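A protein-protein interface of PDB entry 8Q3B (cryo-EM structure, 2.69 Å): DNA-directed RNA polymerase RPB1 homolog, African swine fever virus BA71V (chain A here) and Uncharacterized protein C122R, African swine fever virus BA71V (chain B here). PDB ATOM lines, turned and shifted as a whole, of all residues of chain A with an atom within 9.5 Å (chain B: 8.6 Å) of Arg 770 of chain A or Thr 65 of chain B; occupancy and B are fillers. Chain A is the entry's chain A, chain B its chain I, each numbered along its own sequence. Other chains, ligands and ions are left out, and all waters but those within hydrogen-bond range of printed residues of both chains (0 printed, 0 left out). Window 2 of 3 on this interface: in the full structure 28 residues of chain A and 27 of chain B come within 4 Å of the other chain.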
ATOM      1  N   ILE A 762      20.495 -37.632  18.738  1.00  0.00           N
ATOM      2  CA  ILE A 762      20.807 -36.311  18.207  1.00  0.00           C
ATOM      3  C   ILE A 762      20.764 -35.303  19.348  1.00  0.00           C
ATOM      4  O   ILE A 762      19.712 -35.073  19.953  1.00  0.00           O
ATOM      5  CB  ILE A 762      19.830 -35.926  17.089  1.00  0.00           C
ATOM      6  CG1 ILE A 762      19.847 -36.972  15.969  1.00  0.00           C
ATOM      7  CG2 ILE A 762      20.172 -34.552  16.534  1.00  0.00           C
ATOM      8  CD1 ILE A 762      21.197 -37.166  15.307  1.00  0.00           C
ATOM      9  N   GLN A 763      21.913 -34.697  19.646  1.00  0.00           N
ATOM     10  CA  GLN A 763      21.993 -33.762  20.754  1.00  0.00           C
ATOM     11  C   GLN A 763      21.388 -32.412  20.364  1.00  0.00           C
ATOM     12  O   GLN A 763      21.410 -32.032  19.190  1.00  0.00           O
ATOM     13  CB  GLN A 763      23.443 -33.571  21.186  1.00  0.00           C
ATOM     14  CG  GLN A 763      24.082 -34.819  21.782  1.00  0.00           C
ATOM     15  CD  GLN A 763      23.328 -35.346  22.988  1.00  0.00           C
ATOM     16  OE1 GLN A 763      22.386 -36.125  22.853  1.00  0.00           O
ATOM     17  NE2 GLN A 763      23.743 -34.922  24.177  1.00  0.00           N
ATOM     18  N   PRO A 764      20.839 -31.661  21.332  1.00  0.00           N
ATOM     19  CA  PRO A 764      20.212 -30.375  20.990  1.00  0.00           C
ATOM     20  C   PRO A 764      21.221 -29.284  20.659  1.00  0.00           C
ATOM     21  O   PRO A 764      21.574 -28.473  21.521  1.00  0.00           O
ATOM     22  CB  PRO A 764      19.407 -30.033  22.254  1.00  0.00           C
ATOM     23  CG  PRO A 764      19.310 -31.314  23.019  1.00  0.00           C
ATOM     24  CD  PRO A 764      20.592 -32.012  22.739  1.00  0.00           C
ATOM     25  N   GLN A 765      21.697 -29.255  19.412  1.00  0.00           N
ATOM     26  CA  GLN A 765      22.655 -28.232  19.007  1.00  0.00           C
ATOM     27  C   GLN A 765      21.964 -26.962  18.517  1.00  0.00           C
ATOM     28  O   GLN A 765      22.521 -25.867  18.643  1.00  0.00           O
ATOM     29  CB  GLN A 765      23.576 -28.770  17.907  1.00  0.00           C
ATOM     30  CG  GLN A 765      24.497 -29.965  18.249  1.00  0.00           C
ATOM     31  CD  GLN A 765      25.026 -30.016  19.681  1.00  0.00           C
ATOM     32  OE1 GLN A 765      24.831 -29.103  20.480  1.00  0.00           O
ATOM     33  NE2 GLN A 765      25.715 -31.104  20.002  1.00  0.00           N
ATOM     34  N   PHE A 766      20.761 -27.086  17.952  1.00  0.00           N
ATOM     35  CA  PHE A 766      20.115 -25.933  17.328  1.00  0.00           C
ATOM     36  C   PHE A 766      19.924 -24.800  18.327  1.00  0.00           C
ATOM     37  O   PHE A 766      20.243 -23.641  18.039  1.00  0.00           O
ATOM     38  CB  PHE A 766      18.768 -26.343  16.734  1.00  0.00           C
ATOM     39  CG  PHE A 766      18.024 -25.211  16.085  1.00  0.00           C
ATOM     40  CD1 PHE A 766      18.547 -24.566  14.980  1.00  0.00           C
ATOM     41  CD2 PHE A 766      16.806 -24.789  16.585  1.00  0.00           C
ATOM     42  CE1 PHE A 766      17.866 -23.525  14.383  1.00  0.00           C
ATOM     43  CE2 PHE A 766      16.123 -23.748  15.992  1.00  0.00           C
ATOM     44  CZ  PHE A 766      16.654 -23.116  14.890  1.00  0.00           C
ATOM     45  N   SER A 767      19.403 -25.116  19.507  1.00  0.00           N
ATOM     46  CA  SER A 767      19.133 -24.111  20.524  1.00  0.00           C
ATOM     47  C   SER A 767      19.006 -24.819  21.862  1.00  0.00           C
ATOM     48  O   SER A 767      19.024 -26.050  21.940  1.00  0.00           O
ATOM     49  CB  SER A 767      17.863 -23.318  20.203  1.00  0.00           C
ATOM     50  OG  SER A 767      17.597 -22.355  21.206  1.00  0.00           O
ATOM     51  N   PHE A 768      18.880 -24.025  22.923  1.00  0.00           N
ATOM     52  CA  PHE A 768      18.695 -24.592  24.249  1.00  0.00           C
ATOM     53  C   PHE A 768      17.439 -25.451  24.265  1.00  0.00           C
ATOM     54  O   PHE A 768      16.324 -24.929  24.175  1.00  0.00           O
ATOM     55  CB  PHE A 768      18.607 -23.482  25.298  1.00  0.00           C
ATOM     56  CG  PHE A 768      18.231 -23.969  26.667  1.00  0.00           C
ATOM     57  CD1 PHE A 768      18.988 -24.934  27.307  1.00  0.00           C
ATOM     58  CD2 PHE A 768      17.122 -23.457  27.318  1.00  0.00           C
ATOM     59  CE1 PHE A 768      18.645 -25.382  28.566  1.00  0.00           C
ATOM     60  CE2 PHE A 768      16.775 -23.901  28.577  1.00  0.00           C
ATOM     61  CZ  PHE A 768      17.537 -24.865  29.201  1.00  0.00           C
ATOM     62  N   GLY A 769      17.609 -26.765  24.377  1.00  0.00           N
ATOM     63  CA  GLY A 769      16.483 -27.674  24.406  1.00  0.00           C
ATOM     64  C   GLY A 769      15.889 -28.017  23.058  1.00  0.00           C
ATOM     65  O   GLY A 769      14.828 -28.651  23.018  1.00  0.00           O
ATOM     66  N   ARG A 770      16.527 -27.625  21.957  1.00  0.00           N
ATOM     67  CA  ARG A 770      16.026 -27.904  20.620  1.00  0.00           C
ATOM     68  C   ARG A 770      17.073 -28.660  19.812  1.00  0.00           C
ATOM     69  O   ARG A 770      18.276 -28.423  19.948  1.00  0.00           O
ATOM     70  CB  ARG A 770      15.655 -26.616  19.877  1.00  0.00           C
ATOM     71  CG  ARG A 770      14.607 -25.774  20.570  1.00  0.00           C
ATOM     72  CD  ARG A 770      14.114 -24.657  19.669  1.00  0.00           C
ATOM     73  NE  ARG A 770      13.263 -25.158  18.596  1.00  0.00           N
ATOM     74  CZ  ARG A 770      12.647 -24.390  17.707  1.00  0.00           C
ATOM     75  NH1 ARG A 770      12.772 -23.073  17.726  1.00  0.00           N
ATOM     76  NH2 ARG A 770      11.887 -24.956  16.776  1.00  0.00           N
ATOM     77  N   THR A 771      16.596 -29.570  18.964  1.00  0.00           N
ATOM     78  CA  THR A 771      17.453 -30.299  18.037  1.00  0.00           C
ATOM     79  C   THR A 771      17.342 -29.792  16.608  1.00  0.00           C
ATOM     80  O   THR A 771      18.323 -29.856  15.861  1.00  0.00           O
ATOM     81  CB  THR A 771      17.112 -31.792  18.056  1.00  0.00           C
ATOM     82  OG1 THR A 771      15.774 -31.987  17.586  1.00  0.00           O
ATOM     83  CG2 THR A 771      17.238 -32.356  19.463  1.00  0.00           C
ATOM     84  N   LEU A 772      16.172 -29.293  16.215  1.00  0.00           N
ATOM     85  CA  LEU A 772      15.969 -28.738  14.886  1.00  0.00           C
ATOM     86  C   LEU A 772      14.879 -27.683  14.967  1.00  0.00           C
ATOM     87  O   LEU A 772      14.119 -27.621  15.936  1.00  0.00           O
ATOM     88  CB  LEU A 772      15.584 -29.818  13.868  1.00  0.00           C
ATOM     89  CG  LEU A 772      16.710 -30.634  13.228  1.00  0.00           C
ATOM     90  CD1 LEU A 772      16.126 -31.630  12.242  1.00  0.00           C
ATOM     91  CD2 LEU A 772      17.726 -29.742  12.535  1.00  0.00           C
ATOM     92  N   VAL A 773      14.805 -26.847  13.928  1.00  0.00           N
ATOM     93  CA  VAL A 773      13.783 -25.811  13.874  1.00  0.00           C
ATOM     94  C   VAL A 773      12.380 -26.381  13.752  1.00  0.00           C
ATOM     95  O   VAL A 773      11.405 -25.641  13.912  1.00  0.00           O
ATOM     96  CB  VAL A 773      14.061 -24.850  12.699  1.00  0.00           C
ATOM     97  CG1 VAL A 773      13.726 -25.510  11.371  1.00  0.00           C
ATOM     98  CG2 VAL A 773      13.281 -23.557  12.869  1.00  0.00           C
ATOM     99  N   TYR A 774      12.251 -27.678  13.480  1.00  0.00           N
ATOM    100  CA  TYR A 774      10.955 -28.299  13.249  1.00  0.00           C
ATOM    101  C   TYR A 774      10.318 -28.858  14.512  1.00  0.00           C
ATOM    102  O   TYR A 774       9.180 -29.336  14.447  1.00  0.00           O
ATOM    103  CB  TYR A 774      11.093 -29.423  12.218  1.00  0.00           C
ATOM    104  CG  TYR A 774      11.640 -28.967  10.887  1.00  0.00           C
ATOM    105  CD1 TYR A 774      11.008 -27.968  10.162  1.00  0.00           C
ATOM    106  CD2 TYR A 774      12.787 -29.534  10.356  1.00  0.00           C
ATOM    107  CE1 TYR A 774      11.501 -27.548   8.947  1.00  0.00           C
ATOM    108  CE2 TYR A 774      13.288 -29.120   9.140  1.00  0.00           C
ATOM    109  CZ  TYR A 774      12.642 -28.126   8.440  1.00  0.00           C
ATOM    110  OH  TYR A 774      13.138 -27.710   7.227  1.00  0.00           O
ATOM    111  N   TYR A 775      11.002 -28.811  15.650  1.00  0.00           N
ATOM    112  CA  TYR A 775      10.503 -29.428  16.867  1.00  0.00           C
ATOM    113  C   TYR A 775      10.544 -28.437  18.020  1.00  0.00           C
ATOM    114  O   TYR A 775      11.384 -27.532  18.035  1.00  0.00           O
ATOM    115  CB  TYR A 775      11.326 -30.672  17.225  1.00  0.00           C
ATOM    116  CG  TYR A 775      11.228 -31.764  16.185  1.00  0.00           C
ATOM    117  CD1 TYR A 775      10.036 -32.443  15.976  1.00  0.00           C
ATOM    118  CD2 TYR A 775      12.321 -32.106  15.402  1.00  0.00           C
ATOM    119  CE1 TYR A 775       9.937 -33.435  15.023  1.00  0.00           C
ATOM    120  CE2 TYR A 775      12.231 -33.098  14.447  1.00  0.00           C
ATOM    121  CZ  TYR A 775      11.037 -33.759  14.262  1.00  0.00           C
ATOM    122  OH  TYR A 775      10.940 -34.748  13.312  1.00  0.00           O
ATOM    123  N   PRO A 776       9.652 -28.581  18.999  1.00  0.00           N
ATOM    124  CA  PRO A 776       9.608 -27.615  20.101  1.00  0.00           C
ATOM    125  C   PRO A 776      10.757 -27.825  21.074  1.00  0.00           C
ATOM    126  O   PRO A 776      11.457 -28.838  21.061  1.00  0.00           O
ATOM    127  CB  PRO A 776       8.256 -27.885  20.776  1.00  0.00           C
ATOM    128  CG  PRO A 776       7.594 -28.973  19.981  1.00  0.00           C
ATOM    129  CD  PRO A 776       8.648 -29.642  19.172  1.00  0.00           C
ATOM    130  N   ARG A 777      10.945 -26.826  21.933  1.00  0.00           N
ATOM    131  CA  ARG A 777      11.940 -26.931  22.990  1.00  0.00           C
ATOM    132  C   ARG A 777      11.560 -28.039  23.962  1.00  0.00           C
ATOM    133  O   ARG A 777      10.399 -28.171  24.360  1.00  0.00           O
ATOM    134  CB  ARG A 777      12.064 -25.600  23.729  1.00  0.00           C
ATOM    135  CG  ARG A 777      13.485 -25.229  24.101  1.00  0.00           C
ATOM    136  CD  ARG A 777      13.523 -24.000  24.991  1.00  0.00           C
ATOM    137  NE  ARG A 777      13.094 -22.800  24.283  1.00  0.00           N
ATOM    138  CZ  ARG A 777      13.885 -22.047  23.531  1.00  0.00           C
ATOM    139  NH1 ARG A 777      15.161 -22.347  23.352  1.00  0.00           N
ATOM    140  NH2 ARG A 777      13.383 -20.965  22.943  1.00  0.00           N
ATOM    141  N   PHE A 778      12.552 -28.838  24.353  1.00  0.00           N
ATOM    142  CA  PHE A 778      12.330 -29.962  25.260  1.00  0.00           C
ATOM    143  C   PHE A 778      11.291 -30.929  24.698  1.00  0.00           C
ATOM    144  O   PHE A 778      10.409 -31.406  25.414  1.00  0.00           O
ATOM    145  CB  PHE A 778      11.914 -29.474  26.647  1.00  0.00           C
ATOM    146  CG  PHE A 778      12.717 -28.312  27.145  1.00  0.00           C
ATOM    147  CD1 PHE A 778      14.073 -28.445  27.387  1.00  0.00           C
ATOM    148  CD2 PHE A 778      12.119 -27.086  27.376  1.00  0.00           C
ATOM    149  CE1 PHE A 778      14.815 -27.378  27.846  1.00  0.00           C
ATOM    150  CE2 PHE A 778      12.857 -26.018  27.836  1.00  0.00           C
ATOM    151  CZ  PHE A 778      14.207 -26.165  28.072  1.00  0.00           C
ATOM    152  N   ALA A 779      11.394 -31.219  23.404  1.00  0.00           N
ATOM    153  CA  ALA A 779      10.501 -32.192  22.791  1.00  0.00           C
ATOM    154  C   ALA A 779      10.715 -33.563  23.418  1.00  0.00           C
ATOM    155  O   ALA A 779      11.841 -33.943  23.752  1.00  0.00           O
ATOM    156  CB  ALA A 779      10.741 -32.256  21.284  1.00  0.00           C
ATOM    157  N   ALA A 784      11.963 -36.500  17.436  1.00  0.00           N
ATOM    158  CA  ALA A 784      12.704 -35.255  17.575  1.00  0.00           C
ATOM    159  C   ALA A 784      14.188 -35.471  17.832  1.00  0.00           C
ATOM    160  O   ALA A 784      14.952 -34.504  17.764  1.00  0.00           O
ATOM    161  CB  ALA A 784      12.108 -34.417  18.708  1.00  0.00           C
ATOM    162  N   TYR A 785      14.614 -36.702  18.122  1.00  0.00           N
ATOM    163  CA  TYR A 785      16.004 -36.983  18.464  1.00  0.00           C
ATOM    164  C   TYR A 785      16.652 -37.981  17.513  1.00  0.00           C
ATOM    165  O   TYR A 785      17.697 -38.552  17.839  1.00  0.00           O
ATOM    166  CB  TYR A 785      16.103 -37.481  19.905  1.00  0.00           C
ATOM    167  CG  TYR A 785      15.619 -36.470  20.916  1.00  0.00           C
ATOM    168  CD1 TYR A 785      16.450 -35.444  21.346  1.00  0.00           C
ATOM    169  CD2 TYR A 785      14.334 -36.531  21.431  1.00  0.00           C
ATOM    170  CE1 TYR A 785      16.014 -34.513  22.265  1.00  0.00           C
ATOM    171  CE2 TYR A 785      13.891 -35.604  22.350  1.00  0.00           C
ATOM    172  CZ  TYR A 785      14.735 -34.596  22.764  1.00  0.00           C
ATOM    173  OH  TYR A 785      14.299 -33.669  23.680  1.00  0.00           O
ATOM    174  N   PHE A 803      18.660 -35.805   9.597  1.00  0.00           N
ATOM    175  CA  PHE A 803      19.373 -36.635  10.564  1.00  0.00           C
ATOM    176  C   PHE A 803      20.264 -37.655   9.865  1.00  0.00           C
ATOM    177  O   PHE A 803      21.424 -37.865  10.259  1.00  0.00           O
ATOM    178  CB  PHE A 803      18.372 -37.338  11.478  1.00  0.00           C
ATOM    179  CG  PHE A 803      17.616 -36.406  12.388  1.00  0.00           C
ATOM    180  CD1 PHE A 803      18.249 -35.338  12.998  1.00  0.00           C
ATOM    181  CD2 PHE A 803      16.266 -36.599  12.625  1.00  0.00           C
ATOM    182  CE1 PHE A 803      17.555 -34.487  13.831  1.00  0.00           C
ATOM    183  CE2 PHE A 803      15.568 -35.751  13.458  1.00  0.00           C
ATOM    184  CZ  PHE A 803      16.214 -34.694  14.060  1.00  0.00           C
ATOM    185  N   MET A 806      23.356 -35.878   8.746  1.00  0.00           N
ATOM    186  CA  MET A 806      24.305 -35.712   9.843  1.00  0.00           C
ATOM    187  C   MET A 806      25.110 -36.988  10.053  1.00  0.00           C
ATOM    188  O   MET A 806      26.343 -36.952  10.156  1.00  0.00           O
ATOM    189  CB  MET A 806      23.558 -35.334  11.124  1.00  0.00           C
ATOM    190  CG  MET A 806      22.956 -33.941  11.119  1.00  0.00           C
ATOM    191  SD  MET A 806      22.220 -33.513  12.707  1.00  0.00           S
ATOM    192  CE  MET A 806      21.127 -32.177  12.232  1.00  0.00           C
ATOM    193  N   PHE B  56      14.210 -17.446  32.245  1.00  0.00           N
ATOM    194  CA  PHE B  56      13.686 -18.338  31.216  1.00  0.00           C
ATOM    195  C   PHE B  56      12.329 -18.902  31.612  1.00  0.00           C
ATOM    196  O   PHE B  56      11.416 -18.969  30.785  1.00  0.00           O
ATOM    197  CB  PHE B  56      14.673 -19.472  30.948  1.00  0.00           C
ATOM    198  CG  PHE B  56      14.156 -20.502  29.987  1.00  0.00           C
ATOM    199  CD1 PHE B  56      13.879 -20.164  28.675  1.00  0.00           C
ATOM    200  CD2 PHE B  56      13.939 -21.804  30.398  1.00  0.00           C
ATOM    201  CE1 PHE B  56      13.400 -21.106  27.789  1.00  0.00           C
ATOM    202  CE2 PHE B  56      13.461 -22.750  29.515  1.00  0.00           C
ATOM    203  CZ  PHE B  56      13.191 -22.400  28.210  1.00  0.00           C
ATOM    204  N   ASN B  59       9.670 -16.238  31.234  1.00  0.00           N
ATOM    205  CA  ASN B  59       9.271 -15.976  29.855  1.00  0.00           C
ATOM    206  C   ASN B  59       8.731 -17.202  29.127  1.00  0.00           C
ATOM    207  O   ASN B  59       8.219 -17.060  28.012  1.00  0.00           O
ATOM    208  CB  ASN B  59      10.452 -15.411  29.062  1.00  0.00           C
ATOM    209  CG  ASN B  59      10.863 -14.032  29.530  1.00  0.00           C
ATOM    210  OD1 ASN B  59      10.064 -13.097  29.517  1.00  0.00           O
ATOM    211  ND2 ASN B  59      12.116 -13.898  29.942  1.00  0.00           N
ATOM    212  N   ALA B  60       8.835 -18.391  29.715  1.00  0.00           N
ATOM    213  CA  ALA B  60       8.425 -19.607  29.017  1.00  0.00           C
ATOM    214  C   ALA B  60       7.003 -19.560  28.477  1.00  0.00           C
ATOM    215  O   ALA B  60       6.801 -19.972  27.321  1.00  0.00           O
ATOM    216  CB  ALA B  60       8.595 -20.811  29.953  1.00  0.00           C
ATOM    217  N   PRO B  61       5.994 -19.095  29.217  1.00  0.00           N
ATOM    218  CA  PRO B  61       4.630 -19.118  28.666  1.00  0.00           C
ATOM    219  C   PRO B  61       4.491 -18.342  27.371  1.00  0.00           C
ATOM    220  O   PRO B  61       3.641 -18.685  26.542  1.00  0.00           O
ATOM    221  CB  PRO B  61       3.785 -18.496  29.788  1.00  0.00           C
ATOM    222  CG  PRO B  61       4.608 -18.627  31.019  1.00  0.00           C
ATOM    223  CD  PRO B  61       6.030 -18.543  30.580  1.00  0.00           C
ATOM    224  N   PHE B  62       5.301 -17.306  27.172  1.00  0.00           N
ATOM    225  CA  PHE B  62       5.198 -16.445  26.002  1.00  0.00           C
ATOM    226  C   PHE B  62       6.131 -16.856  24.870  1.00  0.00           C
ATOM    227  O   PHE B  62       6.127 -16.207  23.820  1.00  0.00           O
ATOM    228  CB  PHE B  62       5.486 -14.993  26.400  1.00  0.00           C
ATOM    229  CG  PHE B  62       4.655 -14.508  27.553  1.00  0.00           C
ATOM    230  CD1 PHE B  62       5.034 -14.774  28.858  1.00  0.00           C
ATOM    231  CD2 PHE B  62       3.494 -13.790  27.333  1.00  0.00           C
ATOM    232  CE1 PHE B  62       4.271 -14.332  29.918  1.00  0.00           C
ATOM    233  CE2 PHE B  62       2.728 -13.345  28.391  1.00  0.00           C
ATOM    234  CZ  PHE B  62       3.117 -13.617  29.684  1.00  0.00           C
ATOM    235  N   ASP B  63       6.924 -17.910  25.052  1.00  0.00           N
ATOM    236  CA  ASP B  63       7.851 -18.353  24.019  1.00  0.00           C
ATOM    237  C   ASP B  63       7.151 -19.343  23.096  1.00  0.00           C
ATOM    238  O   ASP B  63       6.739 -20.414  23.559  1.00  0.00           O
ATOM    239  CB  ASP B  63       9.075 -19.001  24.642  1.00  0.00           C
ATOM    240  CG  ASP B  63      10.198 -19.201  23.646  1.00  0.00           C
ATOM    241  OD1 ASP B  63      10.052 -18.767  22.484  1.00  0.00           O
ATOM    242  OD2 ASP B  63      11.230 -19.793  24.024  1.00  0.00           O
ATOM    243  N   PRO B  64       6.991 -19.040  21.804  1.00  0.00           N
ATOM    244  CA  PRO B  64       6.270 -19.976  20.927  1.00  0.00           C
ATOM    245  C   PRO B  64       6.916 -21.345  20.823  1.00  0.00           C
ATOM    246  O   PRO B  64       6.202 -22.344  20.667  1.00  0.00           O
ATOM    247  CB  PRO B  64       6.269 -19.255  19.570  1.00  0.00           C
ATOM    248  CG  PRO B  64       6.530 -17.827  19.882  1.00  0.00           C
ATOM    249  CD  PRO B  64       7.413 -17.828  21.082  1.00  0.00           C
ATOM    250  N   THR B  65       8.240 -21.428  20.905  1.00  0.00           N
ATOM    251  CA  THR B  65       8.961 -22.664  20.625  1.00  0.00           C
ATOM    252  C   THR B  65       9.004 -23.622  21.811  1.00  0.00           C
ATOM    253  O   THR B  65       9.774 -24.585  21.771  1.00  0.00           O
ATOM    254  CB  THR B  65      10.391 -22.349  20.180  1.00  0.00           C
ATOM    255  OG1 THR B  65      11.158 -21.905  21.305  1.00  0.00           O
ATOM    256  CG2 THR B  65      10.397 -21.271  19.108  1.00  0.00           C
ATOM    257  N   ASN B  66       8.209 -23.394  22.851  1.00  0.00           N
ATOM    258  CA  ASN B  66       8.207 -24.251  24.026  1.00  0.00           C
ATOM    259  C   ASN B  66       7.116 -25.310  23.921  1.00  0.00           C
ATOM    260  O   ASN B  66       6.060 -25.088  23.326  1.00  0.00           O
ATOM    261  CB  ASN B  66       8.010 -23.431  25.301  1.00  0.00           C
ATOM    262  CG  ASN B  66       9.322 -22.997  25.919  1.00  0.00           C
ATOM    263  OD1 ASN B  66       9.797 -21.889  25.683  1.00  0.00           O
ATOM    264  ND2 ASN B  66       9.916 -23.876  26.716  1.00  0.00           N
ATOM    265  N   CYS B  67       7.391 -26.471  24.509  1.00  0.00           N
ATOM    266  CA  CYS B  67       6.445 -27.576  24.480  1.00  0.00           C
ATOM    267  C   CYS B  67       5.234 -27.276  25.356  1.00  0.00           C
ATOM    268  O   CYS B  67       5.338 -26.646  26.412  1.00  0.00           O
ATOM    269  CB  CYS B  67       7.118 -28.863  24.952  1.00  0.00           C
ATOM    270  SG  CYS B  67       6.543 -30.356  24.113  1.00  0.00           S
ATOM    271  N   GLN B  68       4.075 -27.751  24.912  1.00  0.00           N
ATOM    272  CA  GLN B  68       2.827 -27.591  25.638  1.00  0.00           C
ATOM    273  C   GLN B  68       2.314 -28.953  26.086  1.00  0.00           C
ATOM    274  O   GLN B  68       2.745 -29.999  25.592  1.00  0.00           O
ATOM    275  CB  GLN B  68       1.766 -26.890  24.778  1.00  0.00           C
ATOM    276  CG  GLN B  68       2.254 -25.637  24.069  1.00  0.00           C
ATOM    277  CD  GLN B  68       2.498 -24.485  25.020  1.00  0.00           C
ATOM    278  OE1 GLN B  68       1.584 -24.023  25.700  1.00  0.00           O
ATOM    279  NE2 GLN B  68       3.738 -24.011  25.071  1.00  0.00           N
ATOM    280  N   THR B  82       2.327 -24.769  29.611  1.00  0.00           N
ATOM    281  CA  THR B  82       3.659 -24.920  29.044  1.00  0.00           C
ATOM    282  C   THR B  82       4.507 -25.820  29.933  1.00  0.00           C
ATOM    283  O   THR B  82       4.508 -25.684  31.159  1.00  0.00           O
ATOM    284  CB  THR B  82       4.327 -23.555  28.884  1.00  0.00           C
ATOM    285  OG1 THR B  82       3.527 -22.728  28.029  1.00  0.00           O
ATOM    286  CG2 THR B  82       5.719 -23.702  28.283  1.00  0.00           C
ATOM    287  N   GLN B  83       5.233 -26.745  29.312  1.00  0.00           N
ATOM    288  CA  GLN B  83       6.060 -27.710  30.023  1.00  0.00           C
ATOM    289  C   GLN B  83       7.522 -27.404  29.732  1.00  0.00           C
ATOM    290  O   GLN B  83       7.912 -27.275  28.568  1.00  0.00           O
ATOM    291  CB  GLN B  83       5.698 -29.140  29.603  1.00  0.00           C
ATOM    292  CG  GLN B  83       6.758 -30.215  29.858  1.00  0.00           C
ATOM    293  CD  GLN B  83       6.733 -31.307  28.807  1.00  0.00           C
ATOM    294  OE1 GLN B  83       5.667 -31.764  28.397  1.00  0.00           O
ATOM    295  NE2 GLN B  83       7.911 -31.727  28.362  1.00  0.00           N
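The side-chain carboxylate (OD2) of Asp 63 of chain B lies within salt-bridge range of the guanidinium group (NH2) of Arg 777 of chain A (2.7 Å).
N of Arg 777 of chain A lies within hydrogen-bond range of O of Thr 65 of chain B, at 2.5 Å.
The backbone NH (N) of Cys 67 of chain B lies close to the backbone carbonyl oxygen (O) of Arg 777 of chain A (3.5 Å).
O of Phe 768 of chain A sits close to NH1 of Arg 777 of chain A (2.9 Å).
O of Gly 769 of chain A lies within hydrogen-bond range of N of Phe 778 of chain A.
The backbone carbonyl oxygen (O) of Val 773 of chain A sits at hydrogen-bond distance from the guanidinium group (NH2) of Arg 770 of chain A, 3.0 Å away.
The side-chain carboxylate of Asp 63 of chain B is in hydrogen-bond range of the side-chain hydroxyl of Thr 65 of chain B (3.4 Å).
O of Asn 66 of chain B sits at hydrogen-bond distance from NE2 of Gln 68 of chain B (3.1 Å).
The backbone carbonyl oxygen of Cys 67 of chain B lies within hydrogen-bond range of the backbone NH of Gln 83 of chain B (2.9 Å).
Phe 768 of chain A touches Phe 56 of chain B (CE2 to CE2, 3.6 Å).
NH1 of Arg 770 of chain A touches CG2 of Thr 65 of chain B, 3.3 Å away.
C of Pro 776 of chain A touches O of Thr 65 of chain B, at 3.5 Å.
CD of Arg 777 of chain A touches CZ of Phe 56 of chain B, at 3.6 Å.
Arg 777 of chain A touches Asn 66 of chain B (NE to OD1, 3.7 Å).
CZ of Phe 56 of chain B touches CE2 of Phe 778 of chain A (3.7 Å).
Phe 778 of chain A touches Asn 66 of chain B.
Gln 83 of chain B touches Phe 778 of chain A (NE2 to O, 3.9 Å).
Ser 767 of chain A touches none of the printed residues of chain B.
Printed residues of chain B within 4 Å of Phe 768 of chain A: Phe 56 (3.6 Å).
No residue of chain B comes within 4 Å of Gly 769 of chain A.
Of chain B, only Thr 65 comes within 4 Å of Arg 770 of chain A.
Thr 771 of chain A touches none of the printed residues of chain B.
Of the printed residues of chain A, Phe 56 of chain B touches Phe 768 (3.6 Å), Arg 777 (3.6 Å) and Phe 778 (3.7 Å).
Asn 59 of chain B touches none of the printed residues of chain A.
Ala 60 of chain B touches none of the printed residues of chain A.
Thr 65 of chain B touches three residues of chain A.
Of chain A, only Arg 777 and Phe 778 come within 4 Å of Asn 66 of chain B.
The nearest printed residue of chain B that does not touch Arg 770 of chain A is Asn 66 of chain B (6.8 Å).
The nearest residue of chain A that does not touch Thr 65 of chain B is Tyr 775 of chain A (5.0 Å).
Hydrophobic or aromatic side chains of chain A that line the printed part of chain B: Phe 768, Pro 776 and Phe 778.
Along chain B the printed residues that touch a printed residue of chain A span positions 56 to 83.
Among the printed residues, 11 pairs touch across the chains.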
